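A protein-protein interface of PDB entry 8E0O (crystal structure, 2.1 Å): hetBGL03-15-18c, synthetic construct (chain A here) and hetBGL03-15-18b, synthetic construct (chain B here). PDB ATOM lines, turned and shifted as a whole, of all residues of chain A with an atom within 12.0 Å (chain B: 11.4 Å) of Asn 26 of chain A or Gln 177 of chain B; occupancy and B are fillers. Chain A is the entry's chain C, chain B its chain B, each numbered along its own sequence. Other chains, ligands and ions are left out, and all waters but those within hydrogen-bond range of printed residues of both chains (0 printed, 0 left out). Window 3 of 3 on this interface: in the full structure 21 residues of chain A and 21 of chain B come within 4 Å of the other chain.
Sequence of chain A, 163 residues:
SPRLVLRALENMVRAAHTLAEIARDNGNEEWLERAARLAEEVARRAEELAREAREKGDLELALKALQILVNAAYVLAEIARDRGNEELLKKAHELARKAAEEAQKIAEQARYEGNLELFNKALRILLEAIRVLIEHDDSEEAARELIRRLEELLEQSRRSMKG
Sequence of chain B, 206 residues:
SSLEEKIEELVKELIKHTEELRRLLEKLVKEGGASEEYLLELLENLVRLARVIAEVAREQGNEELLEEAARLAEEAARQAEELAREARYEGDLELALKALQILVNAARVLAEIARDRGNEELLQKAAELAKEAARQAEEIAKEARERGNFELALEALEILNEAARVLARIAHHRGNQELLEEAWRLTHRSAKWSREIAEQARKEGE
ND1 of His 172 of chain B is in hydrogen-bond range of OD2 of Asp 25 of chain A (3.2 Å). The side-chain amide nitrogen of Gln 177 of chain B lies within hydrogen-bond range of the side-chain amide oxygen of Asn 26 of chain A.
The side-chain amide nitrogen (ND2) of Asn 28 of chain A lies close to the indole nitrogen (NE1) of Trp 31 of chain A, 3.2 Å away.
Among the printed residues, pairs that only touch across the chains: Arg 34 of chain A with Trp 184 of chain B (3.0 Å), Leu 19 of chain A with Trp 184 of chain B (3.3 Å), Ile 22 of chain A with Trp 184 of chain B (3.4 Å), Trp 31 of chain A with Trp 184 of chain B (3.5 Å), Asn 26 of chain A with Leu 180 of chain B (3.5 Å), Ile 22 of chain A with Ala 168 of chain B (3.6 Å) and Ile 22 of chain A with Leu 180 of chain B (3.7 Å).
Asn 26 of chain A touches two residues of chain B. Of chain A, only Asn 26 comes within 4 Å of Gln 177 of chain B. No residue of chain B comes within 4 Å of Ala 23 of chain A. Asp 25 of chain A touches one residue of chain B. No residue of chain B comes within 4 Å of Gly 27 of chain A. No residue of chain B comes within 4 Å of Asn 28 of chain A. Ala 171 of chain B touches none of the printed residues of chain A. No residue of chain A comes within 4 Å of Glu 178 of chain B. No residue of chain A comes within 4 Å of Leu 179 of chain B. Leu 180 of chain B touches just these residues of chain A: Ile 22 and Asn 26. No residue of chain A comes within 4 Å of Glu 181 of chain B. Of the printed residues of chain A, Trp 184 of chain B touches Leu 19 (3.3 Å), Ile 22 (3.4 Å), Trp 31 (3.5 Å) and Arg 34 (3.0 Å). Of the printed residues of chain A, His 172 of chain B touches Asp 25. The nearest residue of chain B that does not touch Asn 26 of chain A is His 172 of chain B (4.8 Å). The nearest printed residue of chain B that does not touch Trp 31 of chain A is Leu 180 of chain B (4.4 Å).
Of the 20 printed residues of chain B, 5 touch a printed residue of chain A. Printed residues of chain B that touch a printed residue of chain A: Ala 168, His 172, Gln 177, Leu 180 and Trp 184. Among the printed residues, no Asp or Glu carboxylate lies within 4 Å of a Lys or Arg side-chain nitrogen of the other chain.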
ATOM      1  N   HIS A  17      -5.667  -7.969   3.619  1.00  0.00           N
ATOM      2  CA  HIS A  17      -5.668  -8.712   4.875  1.00  0.00           C
ATOM      3  C   HIS A  17      -6.057  -7.811   6.040  1.00  0.00           C
ATOM      4  O   HIS A  17      -6.803  -8.226   6.935  1.00  0.00           O
ATOM      5  CB  HIS A  17      -4.293  -9.337   5.113  1.00  0.00           C
ATOM      6  CG  HIS A  17      -4.275 -10.363   6.202  1.00  0.00           C
ATOM      7  ND1 HIS A  17      -4.114 -10.036   7.532  1.00  0.00           N
ATOM      8  CD2 HIS A  17      -4.396 -11.711   6.160  1.00  0.00           C
ATOM      9  CE1 HIS A  17      -4.138 -11.137   8.260  1.00  0.00           C
ATOM     10  NE2 HIS A  17      -4.307 -12.168   7.452  1.00  0.00           N
ATOM     11  N   THR A  18      -5.564  -6.570   6.041  1.00  0.00           N
ATOM     12  CA  THR A  18      -5.933  -5.628   7.093  1.00  0.00           C
ATOM     13  C   THR A  18      -7.405  -5.245   6.996  1.00  0.00           C
ATOM     14  O   THR A  18      -8.098  -5.164   8.017  1.00  0.00           O
ATOM     15  CB  THR A  18      -5.046  -4.384   7.015  1.00  0.00           C
ATOM     16  OG1 THR A  18      -3.681  -4.753   7.249  1.00  0.00           O
ATOM     17  CG2 THR A  18      -5.470  -3.355   8.055  1.00  0.00           C
ATOM     18  N   LEU A  19      -7.902  -5.015   5.778  1.00  0.00           N
ATOM     19  CA  LEU A  19      -9.309  -4.668   5.601  1.00  0.00           C
ATOM     20  C   LEU A  19     -10.221  -5.784   6.097  1.00  0.00           C
ATOM     21  O   LEU A  19     -11.292  -5.520   6.657  1.00  0.00           O
ATOM     22  CB  LEU A  19      -9.596  -4.362   4.130  1.00  0.00           C
ATOM     23  CG  LEU A  19      -9.035  -3.070   3.536  1.00  0.00           C
ATOM     24  CD1 LEU A  19      -9.454  -2.932   2.079  1.00  0.00           C
ATOM     25  CD2 LEU A  19      -9.482  -1.862   4.340  1.00  0.00           C
ATOM     26  N   ALA A  20      -9.815  -7.040   5.898  1.00  0.00           N
ATOM     27  CA  ALA A  20     -10.620  -8.160   6.375  1.00  0.00           C
ATOM     28  C   ALA A  20     -10.616  -8.231   7.895  1.00  0.00           C
ATOM     29  O   ALA A  20     -11.632  -8.579   8.508  1.00  0.00           O
ATOM     30  CB  ALA A  20     -10.109  -9.468   5.772  1.00  0.00           C
ATOM     31  N   GLU A  21      -9.484  -7.902   8.521  1.00  0.00           N
ATOM     32  CA  GLU A  21      -9.416  -7.906   9.977  1.00  0.00           C
ATOM     33  C   GLU A  21     -10.278  -6.801  10.574  1.00  0.00           C
ATOM     34  O   GLU A  21     -10.998  -7.026  11.553  1.00  0.00           O
ATOM     35  CB  GLU A  21      -7.966  -7.760  10.434  1.00  0.00           C
ATOM     36  CG  GLU A  21      -7.671  -8.402  11.780  1.00  0.00           C
ATOM     37  CD  GLU A  21      -6.362  -9.162  11.785  1.00  0.00           C
ATOM     38  OE1 GLU A  21      -6.358 -10.345  11.385  1.00  0.00           O
ATOM     39  OE2 GLU A  21      -5.335  -8.576  12.187  1.00  0.00           O
ATOM     40  N   ILE A  22     -10.213  -5.597   9.997  1.00  0.00           N
ATOM     41  CA  ILE A  22     -11.019  -4.487  10.497  1.00  0.00           C
ATOM     42  C   ILE A  22     -12.501  -4.784  10.313  1.00  0.00           C
ATOM     43  O   ILE A  22     -13.333  -4.429  11.158  1.00  0.00           O
ATOM     44  CB  ILE A  22     -10.615  -3.176   9.796  1.00  0.00           C
ATOM     45  CG1 ILE A  22      -9.132  -2.877  10.028  1.00  0.00           C
ATOM     46  CG2 ILE A  22     -11.464  -2.022  10.298  1.00  0.00           C
ATOM     47  CD1 ILE A  22      -8.677  -1.562   9.430  1.00  0.00           C
ATOM     48  N   ALA A  23     -12.855  -5.442   9.208  1.00  0.00           N
ATOM     49  CA  ALA A  23     -14.254  -5.767   8.956  1.00  0.00           C
ATOM     50  C   ALA A  23     -14.743  -6.868   9.886  1.00  0.00           C
ATOM     51  O   ALA A  23     -15.873  -6.810  10.386  1.00  0.00           O
ATOM     52  CB  ALA A  23     -14.439  -6.174   7.497  1.00  0.00           C
ATOM     53  N   ARG A  24     -13.909  -7.883  10.128  1.00  0.00           N
ATOM     54  CA  ARG A  24     -14.308  -8.965  11.023  1.00  0.00           C
ATOM     55  C   ARG A  24     -14.358  -8.495  12.471  1.00  0.00           C
ATOM     56  O   ARG A  24     -15.223  -8.929  13.241  1.00  0.00           O
ATOM     57  CB  ARG A  24     -13.352 -10.149  10.875  1.00  0.00           C
ATOM     58  N   ASP A  25     -13.439  -7.608  12.859  1.00  0.00           N
ATOM     59  CA  ASP A  25     -13.446  -7.081  14.220  1.00  0.00           C
ATOM     60  C   ASP A  25     -14.691  -6.241  14.473  1.00  0.00           C
ATOM     61  O   ASP A  25     -15.352  -6.384  15.508  1.00  0.00           O
ATOM     62  CB  ASP A  25     -12.180  -6.262  14.470  1.00  0.00           C
ATOM     63  CG  ASP A  25     -11.006  -7.120  14.899  1.00  0.00           C
ATOM     64  OD1 ASP A  25     -11.138  -8.361  14.881  1.00  0.00           O
ATOM     65  OD2 ASP A  25      -9.951  -6.552  15.251  1.00  0.00           O
ATOM     66  N   ASN A  26     -15.028  -5.357  13.533  1.00  0.00           N
ATOM     67  CA  ASN A  26     -16.238  -4.554  13.635  1.00  0.00           C
ATOM     68  C   ASN A  26     -17.498  -5.343  13.306  1.00  0.00           C
ATOM     69  O   ASN A  26     -18.599  -4.882  13.627  1.00  0.00           O
ATOM     70  CB  ASN A  26     -16.133  -3.336  12.709  1.00  0.00           C
ATOM     71  CG  ASN A  26     -17.180  -2.276  13.009  1.00  0.00           C
ATOM     72  OD1 ASN A  26     -16.883  -1.254  13.627  1.00  0.00           O
ATOM     73  ND2 ASN A  26     -18.407  -2.507  12.557  1.00  0.00           N
ATOM     74  N   GLY A  27     -17.368  -6.513  12.686  1.00  0.00           N
ATOM     75  CA  GLY A  27     -18.536  -7.259  12.267  1.00  0.00           C
ATOM     76  C   GLY A  27     -19.272  -6.653  11.096  1.00  0.00           C
ATOM     77  O   GLY A  27     -20.425  -7.013  10.847  1.00  0.00           O
ATOM     78  N   ASN A  28     -18.637  -5.738  10.367  1.00  0.00           N
ATOM     79  CA  ASN A  28     -19.270  -5.091   9.227  1.00  0.00           C
ATOM     80  C   ASN A  28     -19.202  -6.024   8.022  1.00  0.00           C
ATOM     81  O   ASN A  28     -18.114  -6.442   7.612  1.00  0.00           O
ATOM     82  CB  ASN A  28     -18.590  -3.756   8.930  1.00  0.00           C
ATOM     83  CG  ASN A  28     -19.408  -2.873   8.005  1.00  0.00           C
ATOM     84  OD1 ASN A  28     -20.044  -3.351   7.066  1.00  0.00           O
ATOM     85  ND2 ASN A  28     -19.396  -1.571   8.270  1.00  0.00           N
ATOM     86  N   GLU A  29     -20.367  -6.348   7.457  1.00  0.00           N
ATOM     87  CA  GLU A  29     -20.426  -7.324   6.375  1.00  0.00           C
ATOM     88  C   GLU A  29     -20.088  -6.698   5.027  1.00  0.00           C
ATOM     89  O   GLU A  29     -19.351  -7.295   4.233  1.00  0.00           O
ATOM     90  CB  GLU A  29     -21.811  -7.974   6.339  1.00  0.00           C
ATOM     91  CG  GLU A  29     -22.109  -8.762   5.076  1.00  0.00           C
ATOM     92  CD  GLU A  29     -23.595  -8.857   4.793  1.00  0.00           C
ATOM     93  OE1 GLU A  29     -24.177  -7.860   4.316  1.00  0.00           O
ATOM     94  OE2 GLU A  29     -24.182  -9.929   5.051  1.00  0.00           O
ATOM     95  N   GLU A  30     -20.615  -5.502   4.748  1.00  0.00           N
ATOM     96  CA  GLU A  30     -20.269  -4.822   3.504  1.00  0.00           C
ATOM     97  C   GLU A  30     -18.792  -4.456   3.464  1.00  0.00           C
ATOM     98  O   GLU A  30     -18.195  -4.397   2.382  1.00  0.00           O
ATOM     99  CB  GLU A  30     -21.133  -3.573   3.327  1.00  0.00           C
ATOM    100  N   TRP A  31     -18.189  -4.205   4.628  1.00  0.00           N
ATOM    101  CA  TRP A  31     -16.753  -3.963   4.685  1.00  0.00           C
ATOM    102  C   TRP A  31     -15.970  -5.220   4.328  1.00  0.00           C
ATOM    103  O   TRP A  31     -14.947  -5.146   3.638  1.00  0.00           O
ATOM    104  CB  TRP A  31     -16.362  -3.470   6.079  1.00  0.00           C
ATOM    105  CG  TRP A  31     -16.660  -2.025   6.334  1.00  0.00           C
ATOM    106  CD1 TRP A  31     -17.587  -1.251   5.697  1.00  0.00           C
ATOM    107  CD2 TRP A  31     -16.045  -1.185   7.319  1.00  0.00           C
ATOM    108  NE1 TRP A  31     -17.578   0.022   6.216  1.00  0.00           N
ATOM    109  CE2 TRP A  31     -16.641   0.087   7.213  1.00  0.00           C
ATOM    110  CE3 TRP A  31     -15.045  -1.385   8.275  1.00  0.00           C
ATOM    111  CZ2 TRP A  31     -16.268   1.155   8.028  1.00  0.00           C
ATOM    112  CZ3 TRP A  31     -14.677  -0.325   9.082  1.00  0.00           C
ATOM    113  CH2 TRP A  31     -15.287   0.929   8.953  1.00  0.00           C
ATOM    114  N   LEU A  32     -16.437  -6.382   4.794  1.00  0.00           N
ATOM    115  CA  LEU A  32     -15.742  -7.633   4.506  1.00  0.00           C
ATOM    116  C   LEU A  32     -15.783  -7.957   3.019  1.00  0.00           C
ATOM    117  O   LEU A  32     -14.793  -8.437   2.452  1.00  0.00           O
ATOM    118  CB  LEU A  32     -16.354  -8.772   5.321  1.00  0.00           C
ATOM    119  CG  LEU A  32     -15.573 -10.086   5.362  1.00  0.00           C
ATOM    120  CD1 LEU A  32     -14.189  -9.869   5.954  1.00  0.00           C
ATOM    121  CD2 LEU A  32     -16.338 -11.141   6.147  1.00  0.00           C
ATOM    122  N   GLU A  33     -16.923  -7.709   2.372  1.00  0.00           N
ATOM    123  CA  GLU A  33     -17.011  -7.897   0.929  1.00  0.00           C
ATOM    124  C   GLU A  33     -16.042  -6.980   0.195  1.00  0.00           C
ATOM    125  O   GLU A  33     -15.509  -7.350  -0.859  1.00  0.00           O
ATOM    126  CB  GLU A  33     -18.448  -7.658   0.462  1.00  0.00           C
ATOM    127  CG  GLU A  33     -18.651  -7.723  -1.042  1.00  0.00           C
ATOM    128  CD  GLU A  33     -20.085  -7.445  -1.444  1.00  0.00           C
ATOM    129  OE1 GLU A  33     -20.924  -7.227  -0.544  1.00  0.00           O
ATOM    130  OE2 GLU A  33     -20.376  -7.447  -2.658  1.00  0.00           O
ATOM    131  N   ARG A  34     -15.791  -5.789   0.743  1.00  0.00           N
ATOM    132  CA  ARG A  34     -14.826  -4.879   0.140  1.00  0.00           C
ATOM    133  C   ARG A  34     -13.399  -5.386   0.311  1.00  0.00           C
ATOM    134  O   ARG A  34     -12.542  -5.128  -0.543  1.00  0.00           O
ATOM    135  CB  ARG A  34     -14.998  -3.480   0.738  1.00  0.00           C
ATOM    136  CG  ARG A  34     -16.231  -2.774   0.178  1.00  0.00           C
ATOM    137  CD  ARG A  34     -16.220  -1.254   0.304  1.00  0.00           C
ATOM    138  NE  ARG A  34     -17.565  -0.752   0.578  1.00  0.00           N
ATOM    139  CZ  ARG A  34     -17.871   0.127   1.521  1.00  0.00           C
ATOM    140  NH1 ARG A  34     -16.935   0.721   2.242  1.00  0.00           N
ATOM    141  NH2 ARG A  34     -19.148   0.438   1.730  1.00  0.00           N
ATOM    142  N   ALA A  35     -13.134  -6.121   1.392  1.00  0.00           N
ATOM    143  CA  ALA A  35     -11.817  -6.720   1.576  1.00  0.00           C
ATOM    144  C   ALA A  35     -11.627  -7.919   0.659  1.00  0.00           C
ATOM    145  O   ALA A  35     -10.547  -8.104   0.086  1.00  0.00           O
ATOM    146  CB  ALA A  35     -11.625  -7.127   3.036  1.00  0.00           C
ATOM    147  N   ASP A  82     -14.179 -17.808   7.882  1.00  0.00           N
ATOM    148  CA  ASP A  82     -14.886 -17.043   8.900  1.00  0.00           C
ATOM    149  C   ASP A  82     -16.349 -16.836   8.531  1.00  0.00           C
ATOM    150  O   ASP A  82     -17.201 -16.733   9.420  1.00  0.00           O
ATOM    151  CB  ASP A  82     -14.196 -15.696   9.117  1.00  0.00           C
ATOM    152  N   ALA B 164      -1.695   1.627  10.297  1.00  0.00           N
ATOM    153  CA  ALA B 164      -3.149   1.528  10.365  1.00  0.00           C
ATOM    154  C   ALA B 164      -3.595   0.169  10.887  1.00  0.00           C
ATOM    155  O   ALA B 164      -4.650   0.067  11.524  1.00  0.00           O
ATOM    156  CB  ALA B 164      -3.759   1.795   8.989  1.00  0.00           C
ATOM    157  N   LEU B 167      -3.260   0.626  14.646  1.00  0.00           N
ATOM    158  CA  LEU B 167      -4.280   1.534  15.160  1.00  0.00           C
ATOM    159  C   LEU B 167      -5.660   0.888  15.163  1.00  0.00           C
ATOM    160  O   LEU B 167      -6.516   1.257  15.976  1.00  0.00           O
ATOM    161  CB  LEU B 167      -4.303   2.820  14.333  1.00  0.00           C
ATOM    162  CG  LEU B 167      -3.196   3.839  14.607  1.00  0.00           C
ATOM    163  CD1 LEU B 167      -3.299   5.009  13.639  1.00  0.00           C
ATOM    164  CD2 LEU B 167      -3.251   4.322  16.049  1.00  0.00           C
ATOM    165  N   ALA B 168      -5.895  -0.069  14.264  1.00  0.00           N
ATOM    166  CA  ALA B 168      -7.187  -0.743  14.215  1.00  0.00           C
ATOM    167  C   ALA B 168      -7.337  -1.753  15.345  1.00  0.00           C
ATOM    168  O   ALA B 168      -8.411  -1.858  15.948  1.00  0.00           O
ATOM    169  CB  ALA B 168      -7.371  -1.428  12.862  1.00  0.00           C
ATOM    170  N   ARG B 169      -6.273  -2.506  15.643  1.00  0.00           N
ATOM    171  CA  ARG B 169      -6.330  -3.460  16.746  1.00  0.00           C
ATOM    172  C   ARG B 169      -6.534  -2.756  18.080  1.00  0.00           C
ATOM    173  O   ARG B 169      -7.191  -3.300  18.975  1.00  0.00           O
ATOM    174  CB  ARG B 169      -5.057  -4.305  16.777  1.00  0.00           C
ATOM    175  N   ILE B 170      -5.981  -1.551  18.232  1.00  0.00           N
ATOM    176  CA  ILE B 170      -6.232  -0.763  19.433  1.00  0.00           C
ATOM    177  C   ILE B 170      -7.696  -0.348  19.497  1.00  0.00           C
ATOM    178  O   ILE B 170      -8.314  -0.354  20.569  1.00  0.00           O
ATOM    179  CB  ILE B 170      -5.290   0.455  19.472  1.00  0.00           C
ATOM    180  CG1 ILE B 170      -3.880   0.030  19.885  1.00  0.00           C
ATOM    181  CG2 ILE B 170      -5.820   1.524  20.417  1.00  0.00           C
ATOM    182  CD1 ILE B 170      -2.830   1.087  19.632  1.00  0.00           C
ATOM    183  N   ALA B 171      -8.281   0.003  18.348  1.00  0.00           N
ATOM    184  CA  ALA B 171      -9.680   0.414  18.320  1.00  0.00           C
ATOM    185  C   ALA B 171     -10.615  -0.739  18.667  1.00  0.00           C
ATOM    186  O   ALA B 171     -11.662  -0.517  19.286  1.00  0.00           O
ATOM    187  CB  ALA B 171     -10.031   0.989  16.949  1.00  0.00           C
ATOM    188  N   HIS B 172     -10.263  -1.967  18.283  1.00  0.00           N
ATOM    189  CA  HIS B 172     -11.089  -3.113  18.641  1.00  0.00           C
ATOM    190  C   HIS B 172     -10.837  -3.573  20.070  1.00  0.00           C
ATOM    191  O   HIS B 172     -11.768  -4.032  20.742  1.00  0.00           O
ATOM    192  CB  HIS B 172     -10.847  -4.271  17.671  1.00  0.00           C
ATOM    193  CG  HIS B 172     -11.732  -5.454  17.914  1.00  0.00           C
ATOM    194  ND1 HIS B 172     -11.236  -6.719  18.150  1.00  0.00           N
ATOM    195  CD2 HIS B 172     -13.081  -5.564  17.964  1.00  0.00           C
ATOM    196  CE1 HIS B 172     -12.241  -7.557  18.332  1.00  0.00           C
ATOM    197  NE2 HIS B 172     -13.371  -6.880  18.224  1.00  0.00           N
ATOM    198  N   HIS B 173      -9.595  -3.464  20.551  1.00  0.00           N
ATOM    199  CA  HIS B 173      -9.304  -3.825  21.934  1.00  0.00           C
ATOM    200  C   HIS B 173      -9.959  -2.846  22.901  1.00  0.00           C
ATOM    201  O   HIS B 173     -10.569  -3.253  23.896  1.00  0.00           O
ATOM    202  CB  HIS B 173      -7.792  -3.879  22.155  1.00  0.00           C
ATOM    203  N   ARG B 174      -9.842  -1.550  22.623  1.00  0.00           N
ATOM    204  CA  ARG B 174     -10.483  -0.526  23.432  1.00  0.00           C
ATOM    205  C   ARG B 174     -11.903  -0.290  22.918  1.00  0.00           C
ATOM    206  O   ARG B 174     -12.406  -1.015  22.056  1.00  0.00           O
ATOM    207  CB  ARG B 174      -9.649   0.755  23.424  1.00  0.00           C
ATOM    208  N   GLY B 175     -12.566   0.735  23.444  1.00  0.00           N
ATOM    209  CA  GLY B 175     -13.931   1.045  23.081  1.00  0.00           C
ATOM    210  C   GLY B 175     -14.099   2.071  21.983  1.00  0.00           C
ATOM    211  O   GLY B 175     -15.230   2.490  21.715  1.00  0.00           O
ATOM    212  N   ASN B 176     -13.017   2.486  21.332  1.00  0.00           N
ATOM    213  CA  ASN B 176     -13.103   3.505  20.296  1.00  0.00           C
ATOM    214  C   ASN B 176     -13.611   2.891  18.997  1.00  0.00           C
ATOM    215  O   ASN B 176     -13.126   1.842  18.562  1.00  0.00           O
ATOM    216  CB  ASN B 176     -11.739   4.161  20.076  1.00  0.00           C
ATOM    217  CG  ASN B 176     -11.821   5.429  19.238  1.00  0.00           C
ATOM    218  OD1 ASN B 176     -12.692   5.571  18.380  1.00  0.00           O
ATOM    219  ND2 ASN B 176     -10.902   6.355  19.483  1.00  0.00           N
ATOM    220  N   GLN B 177     -14.592   3.550  18.382  1.00  0.00           N
ATOM    221  CA  GLN B 177     -15.081   3.179  17.062  1.00  0.00           C
ATOM    222  C   GLN B 177     -14.655   4.148  15.973  1.00  0.00           C
ATOM    223  O   GLN B 177     -14.522   3.740  14.817  1.00  0.00           O
ATOM    224  CB  GLN B 177     -16.612   3.079  17.068  1.00  0.00           C
ATOM    225  CG  GLN B 177     -17.160   1.870  16.325  1.00  0.00           C
ATOM    226  CD  GLN B 177     -17.577   2.197  14.905  1.00  0.00           C
ATOM    227  OE1 GLN B 177     -17.805   3.359  14.563  1.00  0.00           O
ATOM    228  NE2 GLN B 177     -17.682   1.171  14.067  1.00  0.00           N
ATOM    229  N   GLU B 178     -14.436   5.419  16.317  1.00  0.00           N
ATOM    230  CA  GLU B 178     -13.945   6.386  15.342  1.00  0.00           C
ATOM    231  C   GLU B 178     -12.523   6.060  14.902  1.00  0.00           C
ATOM    232  O   GLU B 178     -12.164   6.298  13.744  1.00  0.00           O
ATOM    233  CB  GLU B 178     -14.019   7.796  15.929  1.00  0.00           C
ATOM    234  CG  GLU B 178     -13.414   8.883  15.059  1.00  0.00           C
ATOM    235  CD  GLU B 178     -12.876  10.042  15.875  1.00  0.00           C
ATOM    236  OE1 GLU B 178     -13.204  10.125  17.078  1.00  0.00           O
ATOM    237  OE2 GLU B 178     -12.124  10.868  15.317  1.00  0.00           O
ATOM    238  N   LEU B 179     -11.704   5.515  15.806  1.00  0.00           N
ATOM    239  CA  LEU B 179     -10.346   5.132  15.436  1.00  0.00           C
ATOM    240  C   LEU B 179     -10.349   3.980  14.440  1.00  0.00           C
ATOM    241  O   LEU B 179      -9.498   3.924  13.545  1.00  0.00           O
ATOM    242  CB  LEU B 179      -9.545   4.761  16.684  1.00  0.00           C
ATOM    243  N   LEU B 180     -11.297   3.050  14.579  1.00  0.00           N
ATOM    244  CA  LEU B 180     -11.425   1.969  13.609  1.00  0.00           C
ATOM    245  C   LEU B 180     -11.826   2.484  12.235  1.00  0.00           C
ATOM    246  O   LEU B 180     -11.543   1.823  11.229  1.00  0.00           O
ATOM    247  CB  LEU B 180     -12.441   0.935  14.101  1.00  0.00           C
ATOM    248  CG  LEU B 180     -12.281  -0.492  13.574  1.00  0.00           C
ATOM    249  CD1 LEU B 180     -10.937  -1.075  13.974  1.00  0.00           C
ATOM    250  CD2 LEU B 180     -13.413  -1.374  14.074  1.00  0.00           C
ATOM    251  N   GLU B 181     -12.475   3.648  12.169  1.00  0.00           N
ATOM    252  CA  GLU B 181     -12.806   4.248  10.882  1.00  0.00           C
ATOM    253  C   GLU B 181     -11.602   4.956  10.274  1.00  0.00           C
ATOM    254  O   GLU B 181     -11.395   4.899   9.056  1.00  0.00           O
ATOM    255  CB  GLU B 181     -13.974   5.221  11.040  1.00  0.00           C
ATOM    256  N   GLU B 182     -10.797   5.626  11.103  1.00  0.00           N
ATOM    257  CA  GLU B 182      -9.608   6.302  10.593  1.00  0.00           C
ATOM    258  C   GLU B 182      -8.570   5.300  10.105  1.00  0.00           C
ATOM    259  O   GLU B 182      -7.978   5.483   9.034  1.00  0.00           O
ATOM    260  CB  GLU B 182      -9.013   7.210  11.668  1.00  0.00           C
ATOM    261  CG  GLU B 182      -7.564   7.599  11.414  1.00  0.00           C
ATOM    262  CD  GLU B 182      -7.421   8.714  10.395  1.00  0.00           C
ATOM    263  OE1 GLU B 182      -6.275   9.138  10.137  1.00  0.00           O
ATOM    264  OE2 GLU B 182      -8.449   9.172   9.853  1.00  0.00           O
ATOM    265  N   ALA B 183      -8.333   4.236  10.877  1.00  0.00           N
ATOM    266  CA  ALA B 183      -7.432   3.184  10.421  1.00  0.00           C
ATOM    267  C   ALA B 183      -7.949   2.529   9.149  1.00  0.00           C
ATOM    268  O   ALA B 183      -7.159   2.022   8.343  1.00  0.00           O
ATOM    269  CB  ALA B 183      -7.242   2.137  11.518  1.00  0.00           C
ATOM    270  N   TRP B 184      -9.268   2.534   8.950  1.00  0.00           N
ATOM    271  CA  TRP B 184      -9.835   1.973   7.732  1.00  0.00           C
ATOM    272  C   TRP B 184      -9.604   2.886   6.535  1.00  0.00           C
ATOM    273  O   TRP B 184      -9.424   2.399   5.413  1.00  0.00           O
ATOM    274  CB  TRP B 184     -11.327   1.715   7.922  1.00  0.00           C
ATOM    275  CG  TRP B 184     -11.831   0.583   7.099  1.00  0.00           C
ATOM    276  CD1 TRP B 184     -11.424  -0.717   7.159  1.00  0.00           C
ATOM    277  CD2 TRP B 184     -12.826   0.645   6.075  1.00  0.00           C
ATOM    278  NE1 TRP B 184     -12.112  -1.472   6.243  1.00  0.00           N
ATOM    279  CE2 TRP B 184     -12.977  -0.659   5.562  1.00  0.00           C
ATOM    280  CE3 TRP B 184     -13.606   1.674   5.543  1.00  0.00           C
ATOM    281  CZ2 TRP B 184     -13.875  -0.959   4.546  1.00  0.00           C
ATOM    282  CZ3 TRP B 184     -14.495   1.374   4.536  1.00  0.00           C
ATOM    283  CH2 TRP B 184     -14.623   0.067   4.048  1.00  0.00           C
ATOM    284  N   ARG B 185      -9.609   4.203   6.751  1.00  0.00           N
ATOM    285  CA  ARG B 185      -9.330   5.128   5.657  1.00  0.00           C
ATOM    286  C   ARG B 185      -7.859   5.087   5.265  1.00  0.00           C
ATOM    287  O   ARG B 185      -7.523   5.202   4.080  1.00  0.00           O
ATOM    288  CB  ARG B 185      -9.745   6.546   6.050  1.00  0.00           C
